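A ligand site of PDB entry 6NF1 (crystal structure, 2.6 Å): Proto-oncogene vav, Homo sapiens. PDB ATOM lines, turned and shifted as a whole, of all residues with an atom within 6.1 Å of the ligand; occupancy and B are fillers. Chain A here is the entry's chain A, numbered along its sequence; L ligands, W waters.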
ATOM      1  N   LYS A 277     -13.723   5.965 -28.864  1.00  0.00           N
ATOM      2  CA  LYS A 277     -15.152   5.903 -28.534  1.00  0.00           C
ATOM      3  C   LYS A 277     -15.515   7.054 -27.591  1.00  0.00           C
ATOM      4  O   LYS A 277     -16.508   7.757 -27.842  1.00  0.00           O
ATOM      5  CB  LYS A 277     -15.552   4.552 -27.910  1.00  0.00           C
ATOM      6  CG  LYS A 277     -17.024   4.214 -28.118  1.00  0.00           C
ATOM      7  CD  LYS A 277     -17.789   4.136 -26.801  1.00  0.00           C
ATOM      8  CE  LYS A 277     -19.097   3.390 -26.956  1.00  0.00           C
ATOM      9  NZ  LYS A 277     -19.616   2.912 -25.655  1.00  0.00           N
ATOM     10  N   PHE A 280     -15.169  10.506 -29.470  1.00  0.00           N
ATOM     11  CA  PHE A 280     -16.283  10.729 -30.395  1.00  0.00           C
ATOM     12  C   PHE A 280     -17.573  11.226 -29.677  1.00  0.00           C
ATOM     13  O   PHE A 280     -18.575  11.435 -30.347  1.00  0.00           O
ATOM     14  CB  PHE A 280     -16.548   9.472 -31.274  1.00  0.00           C
ATOM     15  CG  PHE A 280     -15.503   9.139 -32.340  1.00  0.00           C
ATOM     16  CD1 PHE A 280     -14.717  10.126 -32.908  1.00  0.00           C
ATOM     17  CD2 PHE A 280     -15.350   7.826 -32.792  1.00  0.00           C
ATOM     18  CE1 PHE A 280     -13.761   9.808 -33.886  1.00  0.00           C
ATOM     19  CE2 PHE A 280     -14.407   7.521 -33.787  1.00  0.00           C
ATOM     20  CZ  PHE A 280     -13.616   8.517 -34.320  1.00  0.00           C
ATOM     21  N   LEU A 281     -17.514  11.460 -28.334  1.00  0.00           N
ATOM     22  CA  LEU A 281     -18.659  12.007 -27.575  1.00  0.00           C
ATOM     23  C   LEU A 281     -18.949  13.433 -27.995  1.00  0.00           C
ATOM     24  O   LEU A 281     -20.071  13.882 -27.864  1.00  0.00           O
ATOM     25  CB  LEU A 281     -18.455  11.941 -26.057  1.00  0.00           C
ATOM     26  CG  LEU A 281     -18.704  10.577 -25.405  1.00  0.00           C
ATOM     27  CD1 LEU A 281     -18.182  10.556 -23.989  1.00  0.00           C
ATOM     28  CD2 LEU A 281     -20.178  10.165 -25.476  1.00  0.00           C
ATOM     29  N   VAL A 282     -17.942  14.104 -28.582  1.00  0.00           N
ATOM     30  CA  VAL A 282     -18.029  15.445 -29.136  1.00  0.00           C
ATOM     31  C   VAL A 282     -19.153  15.560 -30.191  1.00  0.00           C
ATOM     32  O   VAL A 282     -19.601  16.668 -30.500  1.00  0.00           O
ATOM     33  CB  VAL A 282     -16.654  15.949 -29.663  1.00  0.00           C
ATOM     34  CG1 VAL A 282     -15.646  16.065 -28.525  1.00  0.00           C
ATOM     35  CG2 VAL A 282     -16.102  15.065 -30.787  1.00  0.00           C
ATOM     36  N   TYR A 283     -19.591  14.392 -30.722  1.00  0.00           N
ATOM     37  CA  TYR A 283     -20.673  14.288 -31.707  1.00  0.00           C
ATOM     38  C   TYR A 283     -22.037  14.608 -31.135  1.00  0.00           C
ATOM     39  O   TYR A 283     -22.909  15.006 -31.908  1.00  0.00           O
ATOM     40  CB  TYR A 283     -20.684  12.930 -32.416  1.00  0.00           C
ATOM     41  CG  TYR A 283     -19.767  12.892 -33.607  1.00  0.00           C
ATOM     42  CD1 TYR A 283     -20.175  13.396 -34.841  1.00  0.00           C
ATOM     43  CD2 TYR A 283     -18.470  12.375 -33.504  1.00  0.00           C
ATOM     44  CE1 TYR A 283     -19.320  13.383 -35.944  1.00  0.00           C
ATOM     45  CE2 TYR A 283     -17.614  12.352 -34.598  1.00  0.00           C
ATOM     46  CZ  TYR A 283     -18.041  12.869 -35.813  1.00  0.00           C
ATOM     47  OH  TYR A 283     -17.216  12.872 -36.905  1.00  0.00           O
ATOM     48  N   GLY A 284     -22.203  14.459 -29.819  1.00  0.00           N
ATOM     49  CA  GLY A 284     -23.453  14.762 -29.126  1.00  0.00           C
ATOM     50  C   GLY A 284     -23.828  16.203 -29.401  1.00  0.00           C
ATOM     51  O   GLY A 284     -24.940  16.487 -29.821  1.00  0.00           O
ATOM     52  N   ARG A 285     -22.845  17.091 -29.260  1.00  0.00           N
ATOM     53  CA  ARG A 285     -23.004  18.507 -29.518  1.00  0.00           C
ATOM     54  C   ARG A 285     -23.357  18.731 -30.988  1.00  0.00           C
ATOM     55  O   ARG A 285     -24.311  19.474 -31.285  1.00  0.00           O
ATOM     56  CB  ARG A 285     -21.737  19.270 -29.090  1.00  0.00           C
ATOM     57  CG  ARG A 285     -21.890  20.777 -29.216  1.00  0.00           C
ATOM     58  CD  ARG A 285     -20.721  21.548 -28.613  1.00  0.00           C
ATOM     59  NE  ARG A 285     -20.391  22.751 -29.392  1.00  0.00           N
ATOM     60  CZ  ARG A 285     -21.070  23.896 -29.358  1.00  0.00           C
ATOM     61  NH1 ARG A 285     -22.148  24.015 -28.574  1.00  0.00           N
ATOM     62  NH2 ARG A 285     -20.706  24.917 -30.122  1.00  0.00           N
ATOM     63  N   TYR A 286     -22.627  18.070 -31.905  1.00  0.00           N
ATOM     64  CA  TYR A 286     -22.848  18.229 -33.334  1.00  0.00           C
ATOM     65  C   TYR A 286     -24.243  17.794 -33.749  1.00  0.00           C
ATOM     66  O   TYR A 286     -24.958  18.591 -34.351  1.00  0.00           O
ATOM     67  CB  TYR A 286     -21.746  17.549 -34.194  1.00  0.00           C
ATOM     68  CG  TYR A 286     -21.809  18.014 -35.633  1.00  0.00           C
ATOM     69  CD1 TYR A 286     -21.203  19.217 -36.026  1.00  0.00           C
ATOM     70  CD2 TYR A 286     -22.553  17.317 -36.580  1.00  0.00           C
ATOM     71  CE1 TYR A 286     -21.296  19.672 -37.344  1.00  0.00           C
ATOM     72  CE2 TYR A 286     -22.695  17.786 -37.886  1.00  0.00           C
ATOM     73  CZ  TYR A 286     -22.052  18.957 -38.267  1.00  0.00           C
ATOM     74  OH  TYR A 286     -22.205  19.420 -39.545  1.00  0.00           O
ATOM     75  N   CYS A 287     -24.638  16.571 -33.368  1.00  0.00           N
ATOM     76  CA  CYS A 287     -25.926  15.955 -33.658  1.00  0.00           C
ATOM     77  C   CYS A 287     -27.129  16.729 -33.098  1.00  0.00           C
ATOM     78  O   CYS A 287     -28.168  16.776 -33.758  1.00  0.00           O
ATOM     79  CB  CYS A 287     -25.939  14.518 -33.176  1.00  0.00           C
ATOM     80  SG  CYS A 287     -24.729  13.471 -34.017  1.00  0.00           S
ATOM     81  N   SER A 288     -26.993  17.300 -31.893  1.00  0.00           N
ATOM     82  CA  SER A 288     -28.068  18.062 -31.256  1.00  0.00           C
ATOM     83  C   SER A 288     -28.350  19.395 -31.908  1.00  0.00           C
ATOM     84  O   SER A 288     -29.484  19.862 -31.857  1.00  0.00           O
ATOM     85  CB  SER A 288     -27.788  18.255 -29.767  1.00  0.00           C
ATOM     86  OG  SER A 288     -26.541  18.893 -29.538  1.00  0.00           O
ATOM     87  N   GLN A 289     -27.332  20.019 -32.511  1.00  0.00           N
ATOM     88  CA  GLN A 289     -27.475  21.345 -33.114  1.00  0.00           C
ATOM     89  C   GLN A 289     -27.487  21.401 -34.652  1.00  0.00           C
ATOM     90  O   GLN A 289     -27.747  22.476 -35.201  1.00  0.00           O
ATOM     91  CB  GLN A 289     -26.370  22.255 -32.544  1.00  0.00           C
ATOM     92  CG  GLN A 289     -26.602  22.655 -31.081  1.00  0.00           C
ATOM     93  CD  GLN A 289     -25.339  23.072 -30.369  1.00  0.00           C
ATOM     94  OE1 GLN A 289     -24.955  22.492 -29.341  1.00  0.00           O
ATOM     95  NE2 GLN A 289     -24.667  24.091 -30.874  1.00  0.00           N
ATOM     96  N   VAL A 336     -20.144   8.539 -38.698  1.00  0.00           N
ATOM     97  CA  VAL A 336     -20.190   7.839 -37.420  1.00  0.00           C
ATOM     98  C   VAL A 336     -21.199   6.649 -37.476  1.00  0.00           C
ATOM     99  O   VAL A 336     -20.897   5.617 -36.874  1.00  0.00           O
ATOM    100  CB  VAL A 336     -20.366   8.781 -36.197  1.00  0.00           C
ATOM    101  CG1 VAL A 336     -21.573   9.703 -36.325  1.00  0.00           C
ATOM    102  CG2 VAL A 336     -20.393   7.995 -34.894  1.00  0.00           C
ATOM    103  N   LEU A 369     -22.265   3.891 -30.524  1.00  0.00           N
ATOM    104  CA  LEU A 369     -22.137   5.227 -31.105  1.00  0.00           C
ATOM    105  C   LEU A 369     -23.251   5.475 -32.126  1.00  0.00           C
ATOM    106  O   LEU A 369     -23.728   6.599 -32.246  1.00  0.00           O
ATOM    107  CB  LEU A 369     -20.767   5.431 -31.761  1.00  0.00           C
ATOM    108  CG  LEU A 369     -19.535   5.570 -30.861  1.00  0.00           C
ATOM    109  CD1 LEU A 369     -18.403   6.188 -31.638  1.00  0.00           C
ATOM    110  CD2 LEU A 369     -19.810   6.441 -29.641  1.00  0.00           C
ATOM    111  N   ALA A 370     -23.676   4.408 -32.854  1.00  0.00           N
ATOM    112  CA  ALA A 370     -24.781   4.486 -33.819  1.00  0.00           C
ATOM    113  C   ALA A 370     -26.126   4.677 -33.066  1.00  0.00           C
ATOM    114  O   ALA A 370     -26.989   5.418 -33.539  1.00  0.00           O
ATOM    115  CB  ALA A 370     -24.816   3.242 -34.692  1.00  0.00           C
ATOM    116  N   CYS A 372     -26.345   6.144 -29.998  1.00  0.00           N
ATOM    117  CA  CYS A 372     -26.137   7.475 -29.451  1.00  0.00           C
ATOM    118  C   CYS A 372     -26.655   8.499 -30.465  1.00  0.00           C
ATOM    119  O   CYS A 372     -27.402   9.412 -30.084  1.00  0.00           O
ATOM    120  CB  CYS A 372     -24.658   7.714 -29.138  1.00  0.00           C
ATOM    121  SG  CYS A 372     -24.082   6.949 -27.597  1.00  0.00           S
ATOM    122  N   VAL A 373     -26.278   8.304 -31.740  1.00  0.00           N
ATOM    123  CA  VAL A 373     -26.708   9.150 -32.859  1.00  0.00           C
ATOM    124  C   VAL A 373     -28.216   9.126 -32.977  1.00  0.00           C
ATOM    125  O   VAL A 373     -28.840  10.188 -33.023  1.00  0.00           O
ATOM    126  CB  VAL A 373     -26.061   8.750 -34.222  1.00  0.00           C
ATOM    127  CG1 VAL A 373     -26.661   9.565 -35.364  1.00  0.00           C
ATOM    128  CG2 VAL A 373     -24.553   8.931 -34.201  1.00  0.00           C
ATOM    129  N   GLU A 375     -30.568   8.186 -30.799  1.00  0.00           N
ATOM    130  CA  GLU A 375     -31.222   8.779 -29.615  1.00  0.00           C
ATOM    131  C   GLU A 375     -31.353  10.294 -29.720  1.00  0.00           C
ATOM    132  O   GLU A 375     -32.396  10.833 -29.348  1.00  0.00           O
ATOM    133  CB  GLU A 375     -30.505   8.419 -28.302  1.00  0.00           C
ATOM    134  CG  GLU A 375     -30.697   6.984 -27.847  1.00  0.00           C
ATOM    135  CD  GLU A 375     -32.101   6.413 -27.783  1.00  0.00           C
ATOM    136  OE1 GLU A 375     -32.223   5.166 -27.896  1.00  0.00           O
ATOM    137  OE2 GLU A 375     -33.081   7.187 -27.622  1.00  0.00           O
ATOM    138  N   VAL A 376     -30.313  10.967 -30.214  1.00  0.00           N
ATOM    139  CA  VAL A 376     -30.320  12.420 -30.379  1.00  0.00           C
ATOM    140  C   VAL A 376     -31.401  12.816 -31.394  1.00  0.00           C
ATOM    141  O   VAL A 376     -32.201  13.696 -31.111  1.00  0.00           O
ATOM    142  CB  VAL A 376     -28.925  13.025 -30.704  1.00  0.00           C
ATOM    143  CG1 VAL A 376     -29.032  14.520 -30.991  1.00  0.00           C
ATOM    144  CG2 VAL A 376     -27.929  12.771 -29.572  1.00  0.00           C
ATOM    145  N   PHE A 526     -31.271  15.816 -18.437  1.00  0.00           N
ATOM    146  CA  PHE A 526     -29.867  16.162 -18.318  1.00  0.00           C
ATOM    147  C   PHE A 526     -29.426  17.016 -19.501  1.00  0.00           C
ATOM    148  O   PHE A 526     -29.714  16.705 -20.664  1.00  0.00           O
ATOM    149  CB  PHE A 526     -28.998  14.888 -18.260  1.00  0.00           C
ATOM    150  CG  PHE A 526     -29.392  13.975 -17.125  1.00  0.00           C
ATOM    151  CD1 PHE A 526     -30.416  13.035 -17.282  1.00  0.00           C
ATOM    152  CD2 PHE A 526     -28.779  14.073 -15.876  1.00  0.00           C
ATOM    153  CE1 PHE A 526     -30.817  12.212 -16.215  1.00  0.00           C
ATOM    154  CE2 PHE A 526     -29.155  13.243 -14.822  1.00  0.00           C
ATOM    155  CZ  PHE A 526     -30.175  12.318 -14.995  1.00  0.00           C
ATOM    156  N   GLU A 527     -28.690  18.088 -19.198  1.00  0.00           N
ATOM    157  CA  GLU A 527     -28.160  19.052 -20.149  1.00  0.00           C
ATOM    158  C   GLU A 527     -26.663  18.942 -20.243  1.00  0.00           C
ATOM    159  O   GLU A 527     -26.051  19.449 -21.174  1.00  0.00           O
ATOM    160  CB  GLU A 527     -28.609  20.446 -19.758  1.00  0.00           C
ATOM    161  CG  GLU A 527     -30.130  20.514 -19.717  1.00  0.00           C
ATOM    162  CD  GLU A 527     -30.742  21.892 -19.757  1.00  0.00           C
ATOM    163  OE1 GLU A 527     -31.969  22.001 -19.525  1.00  0.00           O
ATOM    164  OE2 GLU A 527     -30.008  22.868 -20.005  1.00  0.00           O
ATOM    165  N   GLU A 528     -26.082  18.187 -19.302  1.00  0.00           N
ATOM    166  CA  GLU A 528     -24.656  17.874 -19.282  1.00  0.00           C
ATOM    167  C   GLU A 528     -24.525  16.367 -19.484  1.00  0.00           C
ATOM    168  O   GLU A 528     -25.415  15.607 -19.110  1.00  0.00           O
ATOM    169  CB  GLU A 528     -23.983  18.304 -17.929  1.00  0.00           C
ATOM    170  CG  GLU A 528     -24.039  19.788 -17.600  1.00  0.00           C
ATOM    171  CD  GLU A 528     -23.478  20.753 -18.636  1.00  0.00           C
ATOM    172  OE1 GLU A 528     -22.411  20.445 -19.198  1.00  0.00           O
ATOM    173  OE2 GLU A 528     -24.093  21.824 -18.847  1.00  0.00           O
ATOM    174  N   THR A 529     -23.378  15.943 -20.045  1.00  0.00           N
ATOM    175  CA  THR A 529     -23.012  14.544 -20.338  1.00  0.00           C
ATOM    176  C   THR A 529     -22.922  13.753 -19.030  1.00  0.00           C
ATOM    177  O   THR A 529     -22.009  13.976 -18.236  1.00  0.00           O
ATOM    178  CB  THR A 529     -21.744  14.522 -21.212  1.00  0.00           C
ATOM    179  OG1 THR A 529     -22.005  15.263 -22.406  1.00  0.00           O
ATOM    180  CG2 THR A 529     -21.284  13.131 -21.553  1.00  0.00           C
ATOM    181  N   THR A 530     -23.929  12.903 -18.763  1.00  0.00           N
ATOM    182  CA  THR A 530     -23.948  12.067 -17.575  1.00  0.00           C
ATOM    183  C   THR A 530     -23.971  10.574 -17.955  1.00  0.00           C
ATOM    184  O   THR A 530     -24.482  10.195 -19.010  1.00  0.00           O
ATOM    185  CB  THR A 530     -25.050  12.452 -16.553  1.00  0.00           C
ATOM    186  OG1 THR A 530     -26.339  12.159 -17.073  1.00  0.00           O
ATOM    187  CG2 THR A 530     -24.967  13.913 -16.103  1.00  0.00           C
ATOM    188  N   SER A 531     -23.365   9.762 -17.091  1.00  0.00           N
ATOM    189  CA  SER A 531     -23.282   8.314 -17.245  1.00  0.00           C
ATOM    190  C   SER A 531     -24.081   7.659 -16.140  1.00  0.00           C
ATOM    191  O   SER A 531     -24.183   8.196 -15.038  1.00  0.00           O
ATOM    192  CB  SER A 531     -21.825   7.848 -17.185  1.00  0.00           C
ATOM    193  OG  SER A 531     -21.078   8.313 -18.291  1.00  0.00           O
ATOM    194  N   LEU A 538     -23.495   5.719 -21.242  1.00  0.00           N
ATOM    195  CA  LEU A 538     -24.014   7.071 -21.454  1.00  0.00           C
ATOM    196  C   LEU A 538     -25.529   7.125 -21.361  1.00  0.00           C
ATOM    197  O   LEU A 538     -26.220   6.228 -21.826  1.00  0.00           O
ATOM    198  CB  LEU A 538     -23.530   7.617 -22.828  1.00  0.00           C
ATOM    199  CG  LEU A 538     -23.859   9.083 -23.190  1.00  0.00           C
ATOM    200  CD1 LEU A 538     -22.911  10.043 -22.538  1.00  0.00           C
ATOM    201  CD2 LEU A 538     -23.863   9.308 -24.705  1.00  0.00           C
ATOM    202  N   LEU A 539     -26.047   8.202 -20.750  1.00  0.00           N
ATOM    203  CA  LEU A 539     -27.481   8.464 -20.707  1.00  0.00           C
ATOM    204  C   LEU A 539     -27.724   9.217 -22.015  1.00  0.00           C
ATOM    205  O   LEU A 539     -27.613  10.429 -22.076  1.00  0.00           O
ATOM    206  CB  LEU A 539     -27.824   9.307 -19.457  1.00  0.00           C
ATOM    207  CG  LEU A 539     -28.656   8.579 -18.386  1.00  0.00           C
ATOM    208  CD1 LEU A 539     -27.876   7.444 -17.757  1.00  0.00           C
ATOM    209  CD2 LEU A 539     -29.079   9.524 -17.322  1.00  0.00           C
ATOM    210  N   ARG A 540     -27.938   8.452 -23.092  1.00  0.00           N
ATOM    211  CA  ARG A 540     -28.029   8.900 -24.481  1.00  0.00           C
ATOM    212  C   ARG A 540     -29.211   9.854 -24.803  1.00  0.00           C
ATOM    213  O   ARG A 540     -30.351   9.599 -24.404  1.00  0.00           O
ATOM    214  CB  ARG A 540     -28.059   7.677 -25.420  1.00  0.00           C
ATOM    215  CG  ARG A 540     -26.856   6.727 -25.282  1.00  0.00           C
ATOM    216  CD  ARG A 540     -26.975   5.435 -26.081  1.00  0.00           C
ATOM    217  NE  ARG A 540     -27.347   4.284 -25.252  1.00  0.00           N
ATOM    218  CZ  ARG A 540     -26.495   3.555 -24.540  1.00  0.00           C
ATOM    219  NH1 ARG A 540     -25.201   3.857 -24.526  1.00  0.00           N
ATOM    220  NH2 ARG A 540     -26.930   2.548 -23.808  1.00  0.00           N
ATOM    221  N   GLY A 541     -28.927  10.917 -25.539  1.00  0.00           N
ATOM    222  CA  GLY A 541     -29.967  11.861 -25.948  1.00  0.00           C
ATOM    223  C   GLY A 541     -29.899  13.253 -25.341  1.00  0.00           C
ATOM    224  O   GLY A 541     -28.960  13.593 -24.617  1.00  0.00           O
ATOM    225  N   THR A 542     -30.906  14.068 -25.642  1.00  0.00           N
ATOM    226  CA  THR A 542     -30.939  15.459 -25.180  1.00  0.00           C
ATOM    227  C   THR A 542     -32.195  15.801 -24.364  1.00  0.00           C
ATOM    228  O   THR A 542     -32.337  16.937 -23.912  1.00  0.00           O
ATOM    229  CB  THR A 542     -30.890  16.364 -26.432  1.00  0.00           C
ATOM    230  OG1 THR A 542     -32.011  16.087 -27.291  1.00  0.00           O
ATOM    231  CG2 THR A 542     -29.576  16.254 -27.181  1.00  0.00           C
ATOM    232  N   GLN A 545     -33.535  11.743 -20.623  1.00  0.00           N
ATOM    233  CA  GLN A 545     -32.686  10.584 -20.929  1.00  0.00           C
ATOM    234  C   GLN A 545     -32.829   9.488 -19.885  1.00  0.00           C
ATOM    235  O   GLN A 545     -32.561   8.337 -20.182  1.00  0.00           O
ATOM    236  CB  GLN A 545     -31.209  11.010 -21.051  1.00  0.00           C
ATOM    237  CG  GLN A 545     -30.974  12.108 -22.078  1.00  0.00           C
ATOM    238  CD  GLN A 545     -31.038  13.491 -21.481  1.00  0.00           C
ATOM    239  OE1 GLN A 545     -31.723  13.776 -20.505  1.00  0.00           O
ATOM    240  NE2 GLN A 545     -30.337  14.403 -22.072  1.00  0.00           N
HETATM  241  C1  LIG L   1     -22.183  19.080 -23.888  1.00  0.00           C
HETATM  242  C2  LIG L   1     -25.617  18.807 -25.301  1.00  0.00           C
HETATM  243  C3  LIG L   1     -27.028  18.865 -24.706  1.00  0.00           C
HETATM  244  O1  LIG L   1     -23.143  18.873 -26.296  1.00  0.00           O
HETATM  245  O2  LIG L   1     -25.754  12.376 -21.098  1.00  0.00           O
HETATM  246  C4  LIG L   1     -22.823  12.890 -26.234  1.00  0.00           C
HETATM  247  C5  LIG L   1     -24.478  11.517 -27.565  1.00  0.00           C
HETATM  248  C6  LIG L   1     -25.787  11.244 -27.291  1.00  0.00           C
HETATM  249  C7  LIG L   1     -25.155  12.510 -25.682  1.00  0.00           C
HETATM  250  C8  LIG L   1     -23.633  11.119 -28.709  1.00  0.00           C
HETATM  251  C9  LIG L   1     -24.108  11.236 -30.014  1.00  0.00           C
HETATM  252  C10 LIG L   1     -23.383  10.734 -31.084  1.00  0.00           C
HETATM  253  C11 LIG L   1     -22.160  10.115 -30.886  1.00  0.00           C
HETATM  254  C12 LIG L   1     -21.376   9.568 -32.056  1.00  0.00           C
HETATM  255  C13 LIG L   1     -21.675  10.018 -29.590  1.00  0.00           C
HETATM  256  C14 LIG L   1     -22.388  10.518 -28.512  1.00  0.00           C
HETATM  257  C15 LIG L   1     -25.133  16.746 -24.023  1.00  0.00           C
HETATM  258  S1  LIG L   1     -23.090  18.130 -25.074  1.00  0.00           S
HETATM  259  O3  LIG L   1     -22.580  16.801 -25.100  1.00  0.00           O
HETATM  260  C16 LIG L   1     -22.010  18.446 -22.533  1.00  0.00           C
HETATM  261  N1  LIG L   1     -24.620  18.042 -24.508  1.00  0.00           N
HETATM  262  C17 LIG L   1     -26.479  16.847 -23.331  1.00  0.00           C
HETATM  263  C18 LIG L   1     -27.479  17.480 -24.286  1.00  0.00           C
HETATM  264  C19 LIG L   1     -27.015  15.532 -22.752  1.00  0.00           C
HETATM  265  C20 LIG L   1     -26.090  14.350 -22.482  1.00  0.00           C
HETATM  266  C21 LIG L   1     -26.589  13.509 -21.323  1.00  0.00           C
HETATM  267  N2  LIG L   1     -25.984  13.547 -23.701  1.00  0.00           N
HETATM  268  C22 LIG L   1     -24.905  13.350 -24.483  1.00  0.00           C
HETATM  269  N3  LIG L   1     -24.054  12.338 -26.516  1.00  0.00           N
HETATM  270  C23 LIG L   1     -22.678  13.629 -25.113  1.00  0.00           C
HETATM  271  N4  LIG L   1     -23.693  13.868 -24.234  1.00  0.00           N
HETATM  272  N5  LIG L   1     -26.210  11.857 -26.138  1.00  0.00           N
HETATM  273  O   HOH W   1     -20.723  16.421 -27.252  1.00  0.00           O
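Phe 280 touches the ligand.
Leu 281 touches the ligand (O to C4, 3.3 Å).
Tyr 283 touches the ligand.
Gly 284 touches the ligand.
Val 336 touches the ligand (CG2 to C12, 3.4 Å).
Leu 369 touches the ligand (O to C12, 3.8 Å).
Cys 372 touches the ligand.
CG2 of Val 373 touches C10 of the ligand, at 3.8 Å.
Val 376 touches the ligand (CG2 to C6, 3.5 Å).
O of Phe 526 touches C19 of the ligand, 3.6 Å away.
Glu 527 touches the ligand (O to C17, 3.4 Å).
Glu 528 touches the ligand.
Leu 538 touches the ligand (CD2 to N3, 3.5 Å).
Arg 540 touches the ligand (CA to N5, 3.8 Å).
CG2 of Thr 542 touches C18 of the ligand, 3.8 Å away.
NE2 of Gln 545 touches C19 of the ligand, at 3.6 Å.
Within 4 Å of the ligand: Phe 280, Leu 281, Tyr 283, Gly 284, Arg 285, Val 336, Leu 369, Cys 372, Val 373, Val 376, Phe 526, Glu 527, Glu 528, Thr 529, Thr 530, Leu 538, Leu 539, Arg 540, Gly 541, Thr 542 and Gln 545.
The backbone NH of Leu 539 lies within hydrogen-bond range of the backbone carbonyl oxygen of Thr 530, 3.1 Å away.
O of Gly 541 lies within hydrogen-bond range of NE2 of Gln 545, at 3.0 Å.
The side-chain hydroxyl (OG) of Ser 288 is in hydrogen-bond range of the backbone carbonyl oxygen (O) of Arg 285 (2.9 Å).
The guanidinium group (NH1) of Arg 285 sits at hydrogen-bond distance from the side-chain amide oxygen (OE1) of Gln 289, at 3.3 Å.
The backbone carbonyl oxygen of Tyr 283 is in hydrogen-bond range of the side-chain sulfur of Cys 287, at 3.2 Å.
The backbone carbonyl oxygen (O) of Gly 284 sits at hydrogen-bond distance from the side-chain hydroxyl (OG) of Ser 288.
NE2 of Gln 545 sits at hydrogen-bond distance from O of Phe 526 (2.8 Å).
The side-chain hydroxyl of Thr 529 sits at hydrogen-bond distance from a nitrogen (N4) of the ligand (2.9 Å).
The backbone carbonyl oxygen of Leu 539 lies within hydrogen-bond range of an oxygen (O2) of the ligand, at 2.9 Å.
The backbone NH of Gly 541 is in hydrogen-bond range of a nitrogen (N5) of the ligand, at 2.9 Å.
A nitrogen (N2) of the ligand is in hydrogen-bond range of the backbone carbonyl oxygen (O) of Gly 541 (3.1 Å).
The backbone NH (N) of Thr 530 lies within hydrogen-bond range of an oxygen (O2) of the ligand, at 3.0 Å.
O of Thr 530 is in hydrogen-bond range of O2 of the ligand (3.3 Å).
An oxygen (O1) of the ligand sits close to the backbone NH (N) of Arg 285, 3.5 Å away.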
